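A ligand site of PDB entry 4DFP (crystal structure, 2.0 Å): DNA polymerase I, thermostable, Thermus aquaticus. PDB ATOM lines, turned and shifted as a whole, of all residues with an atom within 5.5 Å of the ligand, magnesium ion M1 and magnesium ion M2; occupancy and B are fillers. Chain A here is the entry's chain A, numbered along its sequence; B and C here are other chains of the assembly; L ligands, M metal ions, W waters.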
ATOM      1  N   ARG A 281     -40.530  11.820  -4.440  1.00  0.00           N
ATOM      2  CA  ARG A 281     -40.264  11.308  -3.108  1.00  0.00           C
ATOM      3  C   ARG A 281     -41.541  11.352  -2.281  1.00  0.00           C
ATOM      4  O   ARG A 281     -42.469  12.094  -2.593  1.00  0.00           O
ATOM      5  CB  ARG A 281     -39.204  12.165  -2.402  1.00  0.00           C
ATOM      6  CG  ARG A 281     -37.781  11.633  -2.484  1.00  0.00           C
ATOM      7  CD  ARG A 281     -36.877  12.408  -1.536  1.00  0.00           C
ATOM      8  NE  ARG A 281     -35.513  11.901  -1.497  1.00  0.00           N
ATOM      9  CZ  ARG A 281     -34.571  12.400  -0.707  1.00  0.00           C
ATOM     10  NH1 ARG A 281     -34.847  13.409   0.101  1.00  0.00           N
ATOM     11  NH2 ARG A 281     -33.348  11.877  -0.719  1.00  0.00           N
ATOM     12  N   ASP A 318     -30.942  -0.288   3.521  1.00  0.00           N
ATOM     13  CA  ASP A 318     -30.528   1.007   2.986  1.00  0.00           C
ATOM     14  C   ASP A 318     -29.760   0.832   1.679  1.00  0.00           C
ATOM     15  O   ASP A 318     -28.701   0.193   1.652  1.00  0.00           O
ATOM     16  CB  ASP A 318     -29.652   1.722   4.014  1.00  0.00           C
ATOM     17  CG  ASP A 318     -29.513   3.206   3.756  1.00  0.00           C
ATOM     18  OD1 ASP A 318     -29.436   3.600   2.569  1.00  0.00           O
ATOM     19  OD2 ASP A 318     -29.486   3.982   4.730  1.00  0.00           O
ATOM     20  N   TYR A 319     -30.289   1.398   0.588  1.00  0.00           N
ATOM     21  CA  TYR A 319     -29.592   1.361  -0.696  1.00  0.00           C
ATOM     22  C   TYR A 319     -28.226   2.011  -0.602  1.00  0.00           C
ATOM     23  O   TYR A 319     -28.061   3.054   0.042  1.00  0.00           O
ATOM     24  CB  TYR A 319     -30.415   2.036  -1.798  1.00  0.00           C
ATOM     25  CG  TYR A 319     -31.530   1.184  -2.390  1.00  0.00           C
ATOM     26  CD1 TYR A 319     -31.248   0.202  -3.324  1.00  0.00           C
ATOM     27  CD2 TYR A 319     -32.857   1.402  -2.050  1.00  0.00           C
ATOM     28  CE1 TYR A 319     -32.259  -0.572  -3.883  1.00  0.00           C
ATOM     29  CE2 TYR A 319     -33.873   0.638  -2.601  1.00  0.00           C
ATOM     30  CZ  TYR A 319     -33.568  -0.340  -3.513  1.00  0.00           C
ATOM     31  OH  TYR A 319     -34.577  -1.105  -4.071  1.00  0.00           O
ATOM     32  N   SER A 320     -27.239   1.385  -1.239  1.00  0.00           N
ATOM     33  CA  SER A 320     -25.872   1.887  -1.232  1.00  0.00           C
ATOM     34  C   SER A 320     -25.659   2.972  -2.285  1.00  0.00           C
ATOM     35  O   SER A 320     -25.810   2.709  -3.477  1.00  0.00           O
ATOM     36  CB  SER A 320     -24.884   0.743  -1.460  1.00  0.00           C
ATOM     37  OG  SER A 320     -23.574   1.252  -1.693  1.00  0.00           O
ATOM     38  N   GLN A 321     -25.312   4.180  -1.827  1.00  0.00           N
ATOM     39  CA  GLN A 321     -24.941   5.290  -2.700  1.00  0.00           C
ATOM     40  C   GLN A 321     -25.934   5.472  -3.846  1.00  0.00           C
ATOM     41  O   GLN A 321     -25.525   5.634  -4.995  1.00  0.00           O
ATOM     42  CB  GLN A 321     -23.539   5.059  -3.274  1.00  0.00           C
ATOM     43  CG  GLN A 321     -22.526   4.552  -2.267  1.00  0.00           C
ATOM     44  CD  GLN A 321     -21.221   4.112  -2.918  1.00  0.00           C
ATOM     45  OE1 GLN A 321     -20.495   4.927  -3.479  1.00  0.00           O
ATOM     46  NE2 GLN A 321     -20.935   2.811  -2.851  1.00  0.00           N
ATOM     47  N   ILE A 322     -27.215   5.444  -3.520  1.00  0.00           N
ATOM     48  CA  ILE A 322     -28.256   5.249  -4.541  1.00  0.00           C
ATOM     49  C   ILE A 322     -28.272   6.258  -5.692  1.00  0.00           C
ATOM     50  O   ILE A 322     -28.353   5.854  -6.851  1.00  0.00           O
ATOM     51  CB  ILE A 322     -29.672   5.068  -3.913  1.00  0.00           C
ATOM     52  CG1 ILE A 322     -30.643   4.541  -4.967  1.00  0.00           C
ATOM     53  CG2 ILE A 322     -30.183   6.358  -3.296  1.00  0.00           C
ATOM     54  CD1 ILE A 322     -30.219   3.220  -5.579  1.00  0.00           C
ATOM     55  N   GLU A 323     -28.153   7.547  -5.388  1.00  0.00           N
ATOM     56  CA  GLU A 323     -28.234   8.555  -6.449  1.00  0.00           C
ATOM     57  C   GLU A 323     -27.011   8.561  -7.365  1.00  0.00           C
ATOM     58  O   GLU A 323     -27.105   8.931  -8.534  1.00  0.00           O
ATOM     59  CB  GLU A 323     -28.518   9.950  -5.866  1.00  0.00           C
ATOM     60  CG  GLU A 323     -29.940  10.096  -5.354  1.00  0.00           C
ATOM     61  CD  GLU A 323     -30.323  11.541  -5.059  1.00  0.00           C
ATOM     62  OE1 GLU A 323     -29.581  12.456  -5.466  1.00  0.00           O
ATOM     63  OE2 GLU A 323     -31.375  11.750  -4.420  1.00  0.00           O
ATOM     64  N   LEU A 324     -25.863   8.145  -6.833  1.00  0.00           N
ATOM     65  CA  LEU A 324     -24.658   8.036  -7.649  1.00  0.00           C
ATOM     66  C   LEU A 324     -24.787   6.872  -8.633  1.00  0.00           C
ATOM     67  O   LEU A 324     -24.354   6.978  -9.777  1.00  0.00           O
ATOM     68  CB  LEU A 324     -23.413   7.854  -6.777  1.00  0.00           C
ATOM     69  CG  LEU A 324     -23.024   9.046  -5.881  1.00  0.00           C
ATOM     70  CD1 LEU A 324     -21.740   8.750  -5.121  1.00  0.00           C
ATOM     71  CD2 LEU A 324     -22.871  10.316  -6.711  1.00  0.00           C
ATOM     72  N   HIS A 347     -18.198   7.677  -1.353  1.00  0.00           N
ATOM     73  CA  HIS A 347     -18.314   8.395  -0.086  1.00  0.00           C
ATOM     74  C   HIS A 347     -17.089   8.156   0.804  1.00  0.00           C
ATOM     75  O   HIS A 347     -16.564   9.089   1.410  1.00  0.00           O
ATOM     76  CB  HIS A 347     -19.587   7.981   0.649  1.00  0.00           C
ATOM     77  CG  HIS A 347     -20.842   8.370  -0.056  1.00  0.00           C
ATOM     78  ND1 HIS A 347     -20.914   9.446  -0.921  1.00  0.00           N
ATOM     79  CD2 HIS A 347     -22.088   7.829  -0.036  1.00  0.00           C
ATOM     80  CE1 HIS A 347     -22.140   9.547  -1.394  1.00  0.00           C
ATOM     81  NE2 HIS A 347     -22.866   8.570  -0.878  1.00  0.00           N
ATOM     82  N   ARG A 367     -17.660   9.632   6.808  1.00  0.00           N
ATOM     83  CA  ARG A 367     -18.294   9.225   5.559  1.00  0.00           C
ATOM     84  C   ARG A 367     -19.590  10.005   5.331  1.00  0.00           C
ATOM     85  O   ARG A 367     -19.912  10.364   4.194  1.00  0.00           O
ATOM     86  CB  ARG A 367     -18.583   7.719   5.573  1.00  0.00           C
ATOM     87  CG  ARG A 367     -19.104   7.167   4.261  1.00  0.00           C
ATOM     88  CD  ARG A 367     -19.257   5.657   4.326  1.00  0.00           C
ATOM     89  NE  ARG A 367     -19.760   5.119   3.071  1.00  0.00           N
ATOM     90  CZ  ARG A 367     -21.053   5.051   2.742  1.00  0.00           C
ATOM     91  NH1 ARG A 367     -21.972   5.495   3.589  1.00  0.00           N
ATOM     92  NH2 ARG A 367     -21.420   4.538   1.575  1.00  0.00           N
ATOM     93  N   ARG A 368     -20.317  10.268   6.409  1.00  0.00           N
ATOM     94  CA  ARG A 368     -21.548  11.043   6.344  1.00  0.00           C
ATOM     95  C   ARG A 368     -21.275  12.452   5.821  1.00  0.00           C
ATOM     96  O   ARG A 368     -22.017  12.969   4.980  1.00  0.00           O
ATOM     97  CB  ARG A 368     -22.212  11.130   7.710  1.00  0.00           C
ATOM     98  CG  ARG A 368     -23.418  12.048   7.745  1.00  0.00           C
ATOM     99  CD  ARG A 368     -23.954  12.217   9.153  1.00  0.00           C
ATOM    100  NE  ARG A 368     -25.159  13.043   9.162  1.00  0.00           N
ATOM    101  CZ  ARG A 368     -26.387  12.586   8.932  1.00  0.00           C
ATOM    102  NH1 ARG A 368     -26.564  11.296   8.669  1.00  0.00           N
ATOM    103  NH2 ARG A 368     -27.427  13.405   8.963  1.00  0.00           N
ATOM    104  N   ALA A 369     -20.207  13.063   6.320  1.00  0.00           N
ATOM    105  CA  ALA A 369     -19.818  14.408   5.894  1.00  0.00           C
ATOM    106  C   ALA A 369     -19.456  14.428   4.411  1.00  0.00           C
ATOM    107  O   ALA A 369     -19.667  15.431   3.732  1.00  0.00           O
ATOM    108  CB  ALA A 369     -18.651  14.904   6.735  1.00  0.00           C
ATOM    109  N   LYS A 371     -20.885  12.860   2.087  1.00  0.00           N
ATOM    110  CA  LYS A 371     -22.100  12.886   1.284  1.00  0.00           C
ATOM    111  C   LYS A 371     -22.481  14.320   0.918  1.00  0.00           C
ATOM    112  O   LYS A 371     -22.993  14.575  -0.176  1.00  0.00           O
ATOM    113  CB  LYS A 371     -23.263  12.220   2.026  1.00  0.00           C
ATOM    114  CG  LYS A 371     -23.044  10.746   2.309  1.00  0.00           C
ATOM    115  CD  LYS A 371     -24.235  10.148   3.056  1.00  0.00           C
ATOM    116  CE  LYS A 371     -24.018   8.665   3.324  1.00  0.00           C
ATOM    117  NZ  LYS A 371     -25.195   8.067   4.029  1.00  0.00           N
ATOM    118  N   THR A 372     -22.230  15.254   1.833  1.00  0.00           N
ATOM    119  CA  THR A 372     -22.464  16.659   1.574  1.00  0.00           C
ATOM    120  C   THR A 372     -21.562  17.141   0.436  1.00  0.00           C
ATOM    121  O   THR A 372     -21.987  17.906  -0.430  1.00  0.00           O
ATOM    122  CB  THR A 372     -22.191  17.527   2.818  1.00  0.00           C
ATOM    123  OG1 THR A 372     -23.116  17.169   3.858  1.00  0.00           O
ATOM    124  CG2 THR A 372     -22.338  18.997   2.507  1.00  0.00           C
ATOM    125  N   PHE A 375     -22.547  14.894  -3.164  1.00  0.00           N
ATOM    126  CA  PHE A 375     -23.821  15.300  -3.747  1.00  0.00           C
ATOM    127  C   PHE A 375     -23.899  16.818  -3.927  1.00  0.00           C
ATOM    128  O   PHE A 375     -24.504  17.301  -4.882  1.00  0.00           O
ATOM    129  CB  PHE A 375     -24.997  14.796  -2.917  1.00  0.00           C
ATOM    130  CG  PHE A 375     -25.104  13.298  -2.879  1.00  0.00           C
ATOM    131  CD1 PHE A 375     -25.349  12.583  -4.050  1.00  0.00           C
ATOM    132  CD2 PHE A 375     -24.961  12.597  -1.694  1.00  0.00           C
ATOM    133  CE1 PHE A 375     -25.443  11.205  -4.019  1.00  0.00           C
ATOM    134  CE2 PHE A 375     -25.061  11.221  -1.670  1.00  0.00           C
ATOM    135  CZ  PHE A 375     -25.296  10.524  -2.833  1.00  0.00           C
ATOM    136  N   GLY A 376     -23.279  17.556  -3.013  1.00  0.00           N
ATOM    137  CA  GLY A 376     -23.243  19.001  -3.097  1.00  0.00           C
ATOM    138  C   GLY A 376     -22.582  19.474  -4.374  1.00  0.00           C
ATOM    139  O   GLY A 376     -23.139  20.293  -5.110  1.00  0.00           O
ATOM    140  N   TYR A 379     -24.545  18.576  -7.598  1.00  0.00           N
ATOM    141  CA  TYR A 379     -25.753  19.358  -7.854  1.00  0.00           C
ATOM    142  C   TYR A 379     -25.514  20.865  -7.861  1.00  0.00           C
ATOM    143  O   TYR A 379     -26.458  21.657  -7.731  1.00  0.00           O
ATOM    144  CB  TYR A 379     -26.854  18.961  -6.868  1.00  0.00           C
ATOM    145  CG  TYR A 379     -27.290  17.520  -7.049  1.00  0.00           C
ATOM    146  CD1 TYR A 379     -27.601  17.030  -8.307  1.00  0.00           C
ATOM    147  CD2 TYR A 379     -27.380  16.652  -5.968  1.00  0.00           C
ATOM    148  CE1 TYR A 379     -28.000  15.715  -8.488  1.00  0.00           C
ATOM    149  CE2 TYR A 379     -27.764  15.342  -6.134  1.00  0.00           C
ATOM    150  CZ  TYR A 379     -28.077  14.874  -7.398  1.00  0.00           C
ATOM    151  OH  TYR A 379     -28.475  13.568  -7.578  1.00  0.00           O
ATOM    152  N   ASN A 458     -31.450  17.687 -11.011  1.00  0.00           N
ATOM    153  CA  ASN A 458     -31.480  16.860  -9.806  1.00  0.00           C
ATOM    154  C   ASN A 458     -32.683  15.930  -9.795  1.00  0.00           C
ATOM    155  O   ASN A 458     -32.593  14.783  -9.352  1.00  0.00           O
ATOM    156  CB  ASN A 458     -31.496  17.732  -8.551  1.00  0.00           C
ATOM    157  CG  ASN A 458     -31.800  16.943  -7.297  1.00  0.00           C
ATOM    158  OD1 ASN A 458     -32.958  16.781  -6.914  1.00  0.00           O
ATOM    159  ND2 ASN A 458     -30.760  16.431  -6.644  1.00  0.00           N
ATOM    160  N   VAL A 491     -37.679   5.809   4.667  1.00  0.00           N
ATOM    161  CA  VAL A 491     -36.920   7.049   4.762  1.00  0.00           C
ATOM    162  C   VAL A 491     -36.170   7.278   3.458  1.00  0.00           C
ATOM    163  O   VAL A 491     -34.943   7.188   3.408  1.00  0.00           O
ATOM    164  CB  VAL A 491     -35.952   7.044   5.968  1.00  0.00           C
ATOM    165  CG1 VAL A 491     -35.410   8.445   6.234  1.00  0.00           C
ATOM    166  CG2 VAL A 491     -36.653   6.520   7.213  1.00  0.00           C
ATOM    167  N   ASP A 493     -34.652   6.243   0.826  1.00  0.00           N
ATOM    168  CA  ASP A 493     -34.034   5.072   0.224  1.00  0.00           C
ATOM    169  C   ASP A 493     -33.760   3.991   1.261  1.00  0.00           C
ATOM    170  O   ASP A 493     -32.958   3.084   1.038  1.00  0.00           O
ATOM    171  CB  ASP A 493     -32.763   5.448  -0.549  1.00  0.00           C
ATOM    172  CG  ASP A 493     -31.553   5.592   0.350  1.00  0.00           C
ATOM    173  OD1 ASP A 493     -30.451   5.248  -0.120  1.00  0.00           O
ATOM    174  OD2 ASP A 493     -31.690   6.056   1.495  1.00  0.00           O
ATOM    175  N   GLU A 494     -34.447   4.108   2.388  1.00  0.00           N
ATOM    176  CA  GLU A 494     -34.328   3.142   3.465  1.00  0.00           C
ATOM    177  C   GLU A 494     -35.694   2.607   3.845  1.00  0.00           C
ATOM    178  O   GLU A 494     -36.687   3.344   3.851  1.00  0.00           O
ATOM    179  CB  GLU A 494     -33.674   3.803   4.679  1.00  0.00           C
ATOM    180  CG  GLU A 494     -33.679   2.957   5.940  1.00  0.00           C
ATOM    181  CD  GLU A 494     -33.216   3.732   7.159  1.00  0.00           C
ATOM    182  OE1 GLU A 494     -32.890   4.920   7.020  1.00  0.00           O
ATOM    183  OE2 GLU A 494     -33.193   3.145   8.265  1.00  0.00           O
ATOM    184  N   LYS A 539     -28.915  -0.159  12.198  1.00  0.00           N
ATOM    185  CA  LYS A 539     -28.170   0.429  11.085  1.00  0.00           C
ATOM    186  C   LYS A 539     -26.665   0.352  11.307  1.00  0.00           C
ATOM    187  O   LYS A 539     -25.886   0.892  10.518  1.00  0.00           O
ATOM    188  CB  LYS A 539     -28.607   1.869  10.819  1.00  0.00           C
ATOM    189  CG  LYS A 539     -30.023   1.996  10.281  1.00  0.00           C
ATOM    190  CD  LYS A 539     -30.217   3.299   9.514  1.00  0.00           C
ATOM    191  CE  LYS A 539     -29.433   3.294   8.211  1.00  0.00           C
ATOM    192  NZ  LYS A 539     -29.667   4.517   7.402  1.00  0.00           N
ATOM    193  P    DC B   4     -24.364  26.995  -2.862  1.00  0.00           P
ATOM    194  OP1  DC B   4     -24.793  27.254  -1.476  1.00  0.00           O
ATOM    195  OP2  DC B   4     -22.958  27.256  -3.258  1.00  0.00           O
ATOM    196  O5'  DC B   4     -24.688  25.468  -3.231  1.00  0.00           O
ATOM    197  C5'  DC B   4     -26.030  25.018  -3.165  1.00  0.00           C
ATOM    198  C4'  DC B   4     -26.262  23.845  -4.108  1.00  0.00           C
ATOM    199  O4'  DC B   4     -25.359  22.767  -3.766  1.00  0.00           O
ATOM    200  C3'  DC B   4     -27.657  23.251  -4.015  1.00  0.00           C
ATOM    201  O3'  DC B   4     -28.507  23.901  -4.955  1.00  0.00           O
ATOM    202  C2'  DC B   4     -27.416  21.792  -4.403  1.00  0.00           C
ATOM    203  C1'  DC B   4     -26.038  21.526  -3.811  1.00  0.00           C
ATOM    204  N1   DC B   4     -26.040  20.949  -2.435  1.00  0.00           N
ATOM    205  C2   DC B   4     -26.448  19.622  -2.227  1.00  0.00           C
ATOM    206  O2   DC B   4     -26.793  18.948  -3.206  1.00  0.00           O
ATOM    207  N3   DC B   4     -26.434  19.120  -0.975  1.00  0.00           N
ATOM    208  C4   DC B   4     -26.054  19.886   0.052  1.00  0.00           C
ATOM    209  N4   DC B   4     -26.064  19.340   1.273  1.00  0.00           N
ATOM    210  C5   DC B   4     -25.642  21.231  -0.127  1.00  0.00           C
ATOM    211  C6   DC B   4     -25.652  21.721  -1.373  1.00  0.00           C
ATOM    212  P    DG B   5     -29.986  24.343  -4.518  1.00  0.00           P
ATOM    213  OP1  DG B   5     -30.487  25.318  -5.506  1.00  0.00           O
ATOM    214  OP2  DG B   5     -29.958  24.700  -3.080  1.00  0.00           O
ATOM    215  O5'  DG B   5     -30.835  22.992  -4.656  1.00  0.00           O
ATOM    216  C5'  DG B   5     -31.003  22.400  -5.939  1.00  0.00           C
ATOM    217  C4'  DG B   5     -31.533  20.982  -5.808  1.00  0.00           C
ATOM    218  O4'  DG B   5     -30.542  20.162  -5.139  1.00  0.00           O
ATOM    219  C3'  DG B   5     -32.796  20.836  -4.965  1.00  0.00           C
ATOM    220  O3'  DG B   5     -33.944  21.062  -5.763  1.00  0.00           O
ATOM    221  C2'  DG B   5     -32.694  19.388  -4.518  1.00  0.00           C
ATOM    222  C1'  DG B   5     -31.191  19.202  -4.338  1.00  0.00           C
ATOM    223  N9   DG B   5     -30.759  19.326  -2.945  1.00  0.00           N
ATOM    224  C8   DG B   5     -30.072  20.369  -2.381  1.00  0.00           C
ATOM    225  N7   DG B   5     -29.824  20.193  -1.107  1.00  0.00           N
ATOM    226  C5   DG B   5     -30.385  18.958  -0.824  1.00  0.00           C
ATOM    227  C6   DG B   5     -30.436  18.227   0.386  1.00  0.00           C
ATOM    228  O6   DG B   5     -29.971  18.536   1.500  1.00  0.00           O
ATOM    229  N1   DG B   5     -31.103  17.011   0.237  1.00  0.00           N
ATOM    230  C2   DG B   5     -31.659  16.562  -0.943  1.00  0.00           C
ATOM    231  N2   DG B   5     -32.264  15.361  -0.892  1.00  0.00           N
ATOM    232  N3   DG B   5     -31.621  17.230  -2.086  1.00  0.00           N
ATOM    233  C4   DG B   5     -30.967  18.419  -1.945  1.00  0.00           C
ATOM    234  N1  DOC C  12     -31.570  13.068   3.279  1.00  0.00           N
ATOM    235  C2  DOC C  12     -31.598  14.018   2.293  1.00  0.00           C
ATOM    236  N3  DOC C  12     -30.862  15.158   2.425  1.00  0.00           N
ATOM    237  C4  DOC C  12     -30.086  15.398   3.516  1.00  0.00           C
ATOM    238  C5  DOC C  12     -30.051  14.444   4.537  1.00  0.00           C
ATOM    239  C6  DOC C  12     -30.812  13.259   4.402  1.00  0.00           C
ATOM    240  O2  DOC C  12     -32.275  13.863   1.286  1.00  0.00           O
ATOM    241  N4  DOC C  12     -29.326  16.607   3.616  1.00  0.00           N
ATOM    242  C1' DOC C  12     -32.345  11.853   3.178  1.00  0.00           C
ATOM    243  C2' DOC C  12     -31.634  10.747   2.503  1.00  0.00           C
ATOM    244  C3' DOC C  12     -31.312   9.777   3.568  1.00  0.00           C
ATOM    245  C4' DOC C  12     -32.366   9.976   4.547  1.00  0.00           C
ATOM    246  O4' DOC C  12     -32.735  11.390   4.450  1.00  0.00           O
ATOM    247  C5' DOC C  12     -31.858   9.697   5.881  1.00  0.00           C
ATOM    248  O5' DOC C  12     -30.696  10.375   6.280  1.00  0.00           O
ATOM    249  P   DOC C  12     -30.294  10.398   7.773  1.00  0.00           P
ATOM    250  OP1 DOC C  12     -30.402   8.976   8.417  1.00  0.00           O
ATOM    251  OP2 DOC C  12     -28.855  11.022   7.859  1.00  0.00           O
HETATM  252  O1  LIG L   1     -26.696  16.253   1.361  1.00  0.00           O
HETATM  253  C1  LIG L   1     -27.345  15.770   0.405  1.00  0.00           C
HETATM  254  N1  LIG L   1     -27.577  16.497  -0.702  1.00  0.00           N
HETATM  255  C2  LIG L   1     -28.277  15.980  -1.745  1.00  0.00           C
HETATM  256  N2  LIG L   1     -28.491  16.722  -2.851  1.00  0.00           N
HETATM  257  N3  LIG L   1     -28.758  14.720  -1.704  1.00  0.00           N
HETATM  258  C3  LIG L   1     -27.828  14.469   0.465  1.00  0.00           C
HETATM  259  C4  LIG L   1     -28.558  13.950  -0.607  1.00  0.00           C
HETATM  260  C5  LIG L   1     -27.842  13.430   1.367  1.00  0.00           C
HETATM  261  C6  LIG L   1     -27.257  13.429   2.577  1.00  0.00           C
HETATM  262  C7  LIG L   1     -26.740  13.422   3.637  1.00  0.00           C
HETATM  263  C8  LIG L   1     -26.078  13.346   4.949  1.00  0.00           C
HETATM  264  C9  LIG L   1     -25.018  14.441   5.123  1.00  0.00           C
HETATM  265  C10 LIG L   1     -25.663  15.819   5.284  1.00  0.00           C
HETATM  266  N4  LIG L   1     -25.953  16.386   3.975  1.00  0.00           N
HETATM  267  C11 LIG L   1     -28.499  12.324   0.898  1.00  0.00           C
HETATM  268  N5  LIG L   1     -28.942  12.694  -0.317  1.00  0.00           N
HETATM  269  C12 LIG L   1     -29.696  11.812  -1.240  1.00  0.00           C
HETATM  270  C13 LIG L   1     -28.649  11.135  -2.106  1.00  0.00           C
HETATM  271  C14 LIG L   1     -28.591   9.714  -1.581  1.00  0.00           C
HETATM  272  O2  LIG L   1     -28.343   8.809  -2.659  1.00  0.00           O
HETATM  273  O3  LIG L   1     -30.381  10.792  -0.507  1.00  0.00           O
HETATM  274  C15 LIG L   1     -29.970   9.505  -0.969  1.00  0.00           C
HETATM  275  C16 LIG L   1     -29.950   8.516   0.184  1.00  0.00           C
HETATM  276  O4  LIG L   1     -29.160   9.074   1.238  1.00  0.00           O
HETATM  277  P1  LIG L   1     -28.110   8.160   2.037  1.00  0.00           P
HETATM  278  O5  LIG L   1     -27.778   8.868   3.336  1.00  0.00           O
HETATM  279  O6  LIG L   1     -28.524   6.712   2.060  1.00  0.00           O
HETATM  280  O7  LIG L   1     -26.844   8.354   1.076  1.00  0.00           O
HETATM  281  P2  LIG L   1     -26.331   7.178   0.104  1.00  0.00           P
HETATM  282  O8  LIG L   1     -27.437   6.167  -0.101  1.00  0.00           O
HETATM  283  O9  LIG L   1     -25.719   7.853  -1.097  1.00  0.00           O
HETATM  284  O10 LIG L   1     -25.151   6.577   1.022  1.00  0.00           O
HETATM  285  P3  LIG L   1     -25.200   5.101   1.664  1.00  0.00           P
HETATM  286  O11 LIG L   1     -24.500   4.234   0.656  1.00  0.00           O
HETATM  287  O12 LIG L   1     -24.457   5.284   2.971  1.00  0.00           O
HETATM  288  O13 LIG L   1     -26.672   4.806   1.845  1.00  0.00           O
HETATM  289 MG    MG M   1     -28.831   4.825   0.975  1.00  0.00          MG
HETATM  290 MG    MG M   2     -30.725   6.284   3.424  1.00  0.00          MG
HETATM  291  O   HOH W   1     -27.287  10.330   5.658  1.00  0.00           O
HETATM  292  O   HOH W   2     -26.955   5.363   4.865  1.00  0.00           O
HETATM  293  O   HOH W   3     -28.823   7.351   5.630  1.00  0.00           O
HETATM  294  O   HOH W   4     -32.283   6.652   4.670  1.00  0.00           O
HETATM  295  O   HOH W   5     -26.710   1.868   2.507  1.00  0.00           O
HETATM  296  O   HOH W   6     -30.756  14.612  -4.131  1.00  0.00           O
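Magnesium ion M1 is bound by OD1 of Asp 493 (2.0 Å).
Magnesium ion M1 is bound by OD1 of Asp 318, at 2.1 Å.
The backbone carbonyl oxygen (O) of Tyr 319 binds magnesium ion M1, at 2.1 Å.
An oxygen (O6) of the ligand is bound to magnesium ion M1 (2.2 Å).
Magnesium ion M1 is bound by O8 of the ligand (2.2 Å).
An oxygen (O13) of the ligand is bound to magnesium ion M1.
NZ of Lys 539 is in salt-bridge range of OD2 of Asp 318, 2.7 Å away.
The side-chain hydroxyl (OG) of Ser 320 lies within hydrogen-bond range of the side-chain amide nitrogen (NE2) of Gln 321 (3.3 Å).
The side-chain carboxylate (OE1) of Glu 323 is in hydrogen-bond range of the side-chain hydroxyl (OH) of Tyr 379 (2.6 Å).
The guanidinium group (NH1) of Arg 281 sits at hydrogen-bond distance from N2 of DG 5 of chain B (3.4 Å).
N2 of DG 5 of chain B lies close to O2 of DOC 12 of chain C (2.6 Å).
NH1 of Arg 281 lies within hydrogen-bond range of O2 of DOC 12 of chain C (2.9 Å).
OP2 of DOC 12 of chain C lies within salt-bridge range of the guanidinium group of Arg 368, at 2.4 Å.
Magnesium ion M2 is bound by water W4 (2.0 Å) and the side-chain carboxylate of Asp 493 (2.2 Å).
Slightly farther from magnesium ion M2 lies an oxygen (O6) of the ligand (2.6 Å).
CA of Ser 320 touches O11 of the ligand, 3.3 Å away.
Ile 322 touches the ligand.
O of Arg 368 touches C9 of the ligand, at 3.3 Å.
CZ of Phe 375 touches O9 of the ligand, at 3.2 Å.
Tyr 379 touches the ligand.
Hydrophobic or aromatic side chains that line the ligand: Ile 322, His 347, Phe 375 and Tyr 379.
Within 4 Å of the ligand: Arg 281, Asp 318, Tyr 319, Ser 320, Gln 321, Ile 322, Glu 323, His 347, Arg 367, Arg 368, Lys 371, Thr 372, Phe 375, Tyr 379, Asp 493, DC 4 of chain B, DG 5 of chain B and DOC 12 of chain C.
NH1 of Arg 367 is in salt-bridge range of O12 of the ligand (2.6 Å).
O11 of the ligand is in hydrogen-bond range of N of Gln 321, 2.6 Å away.
NZ of Lys 371 lies within salt-bridge range of O5 of the ligand (2.8 Å).
O2 of DC 4 of chain B sits at hydrogen-bond distance from a nitrogen (N2) of the ligand.
The side-chain hydroxyl (OG1) of Thr 372 lies within hydrogen-bond range of a nitrogen (N4) of the ligand, 2.9 Å away.
An oxygen (O9) of the ligand sits at hydrogen-bond distance from a ring nitrogen (NE2) of His 347 (2.9 Å).
N of Glu 323 is in hydrogen-bond range of O2 of the ligand.
A nitrogen (N2) of the ligand lies close to N3 of DG 5 of chain B (3.3 Å).
O3 of the ligand is in hydrogen-bond range of NH2 of Arg 281, at 3.2 Å.
N4 of DOC 12 of chain C sits at hydrogen-bond distance from N4 of the ligand (3.4 Å).
Water W4 lies within hydrogen-bond range of the side-chain carboxylate (OE1) of Glu 494 and the backbone carbonyl oxygen (O) of Val 491.
Water W1 lies within hydrogen-bond range of an oxygen (O5) of the ligand (2.8 Å), OP2 of DOC 12 of chain C (2.8 Å), the guanidinium group of Arg 368 (3.2 Å) and the side-chain amino group of Lys 371 (3.5 Å).
Water W3 lies within hydrogen-bond range of an oxygen (O5) of the ligand (2.9 Å) and the side-chain amino group (NZ) of Lys 539 (3.4 Å).
Water W2 lies within hydrogen-bond range of OD2 of Asp 318 (2.9 Å), O12 of the ligand (3.1 Å) and NZ of Lys 371 (3.3 Å).
Residues that only touch magnesium ion M2: DOC 12 of chain C (3.5 Å).
The nearest printed residue that does not touch magnesium ion M2 is Glu 494 (4.1 Å).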
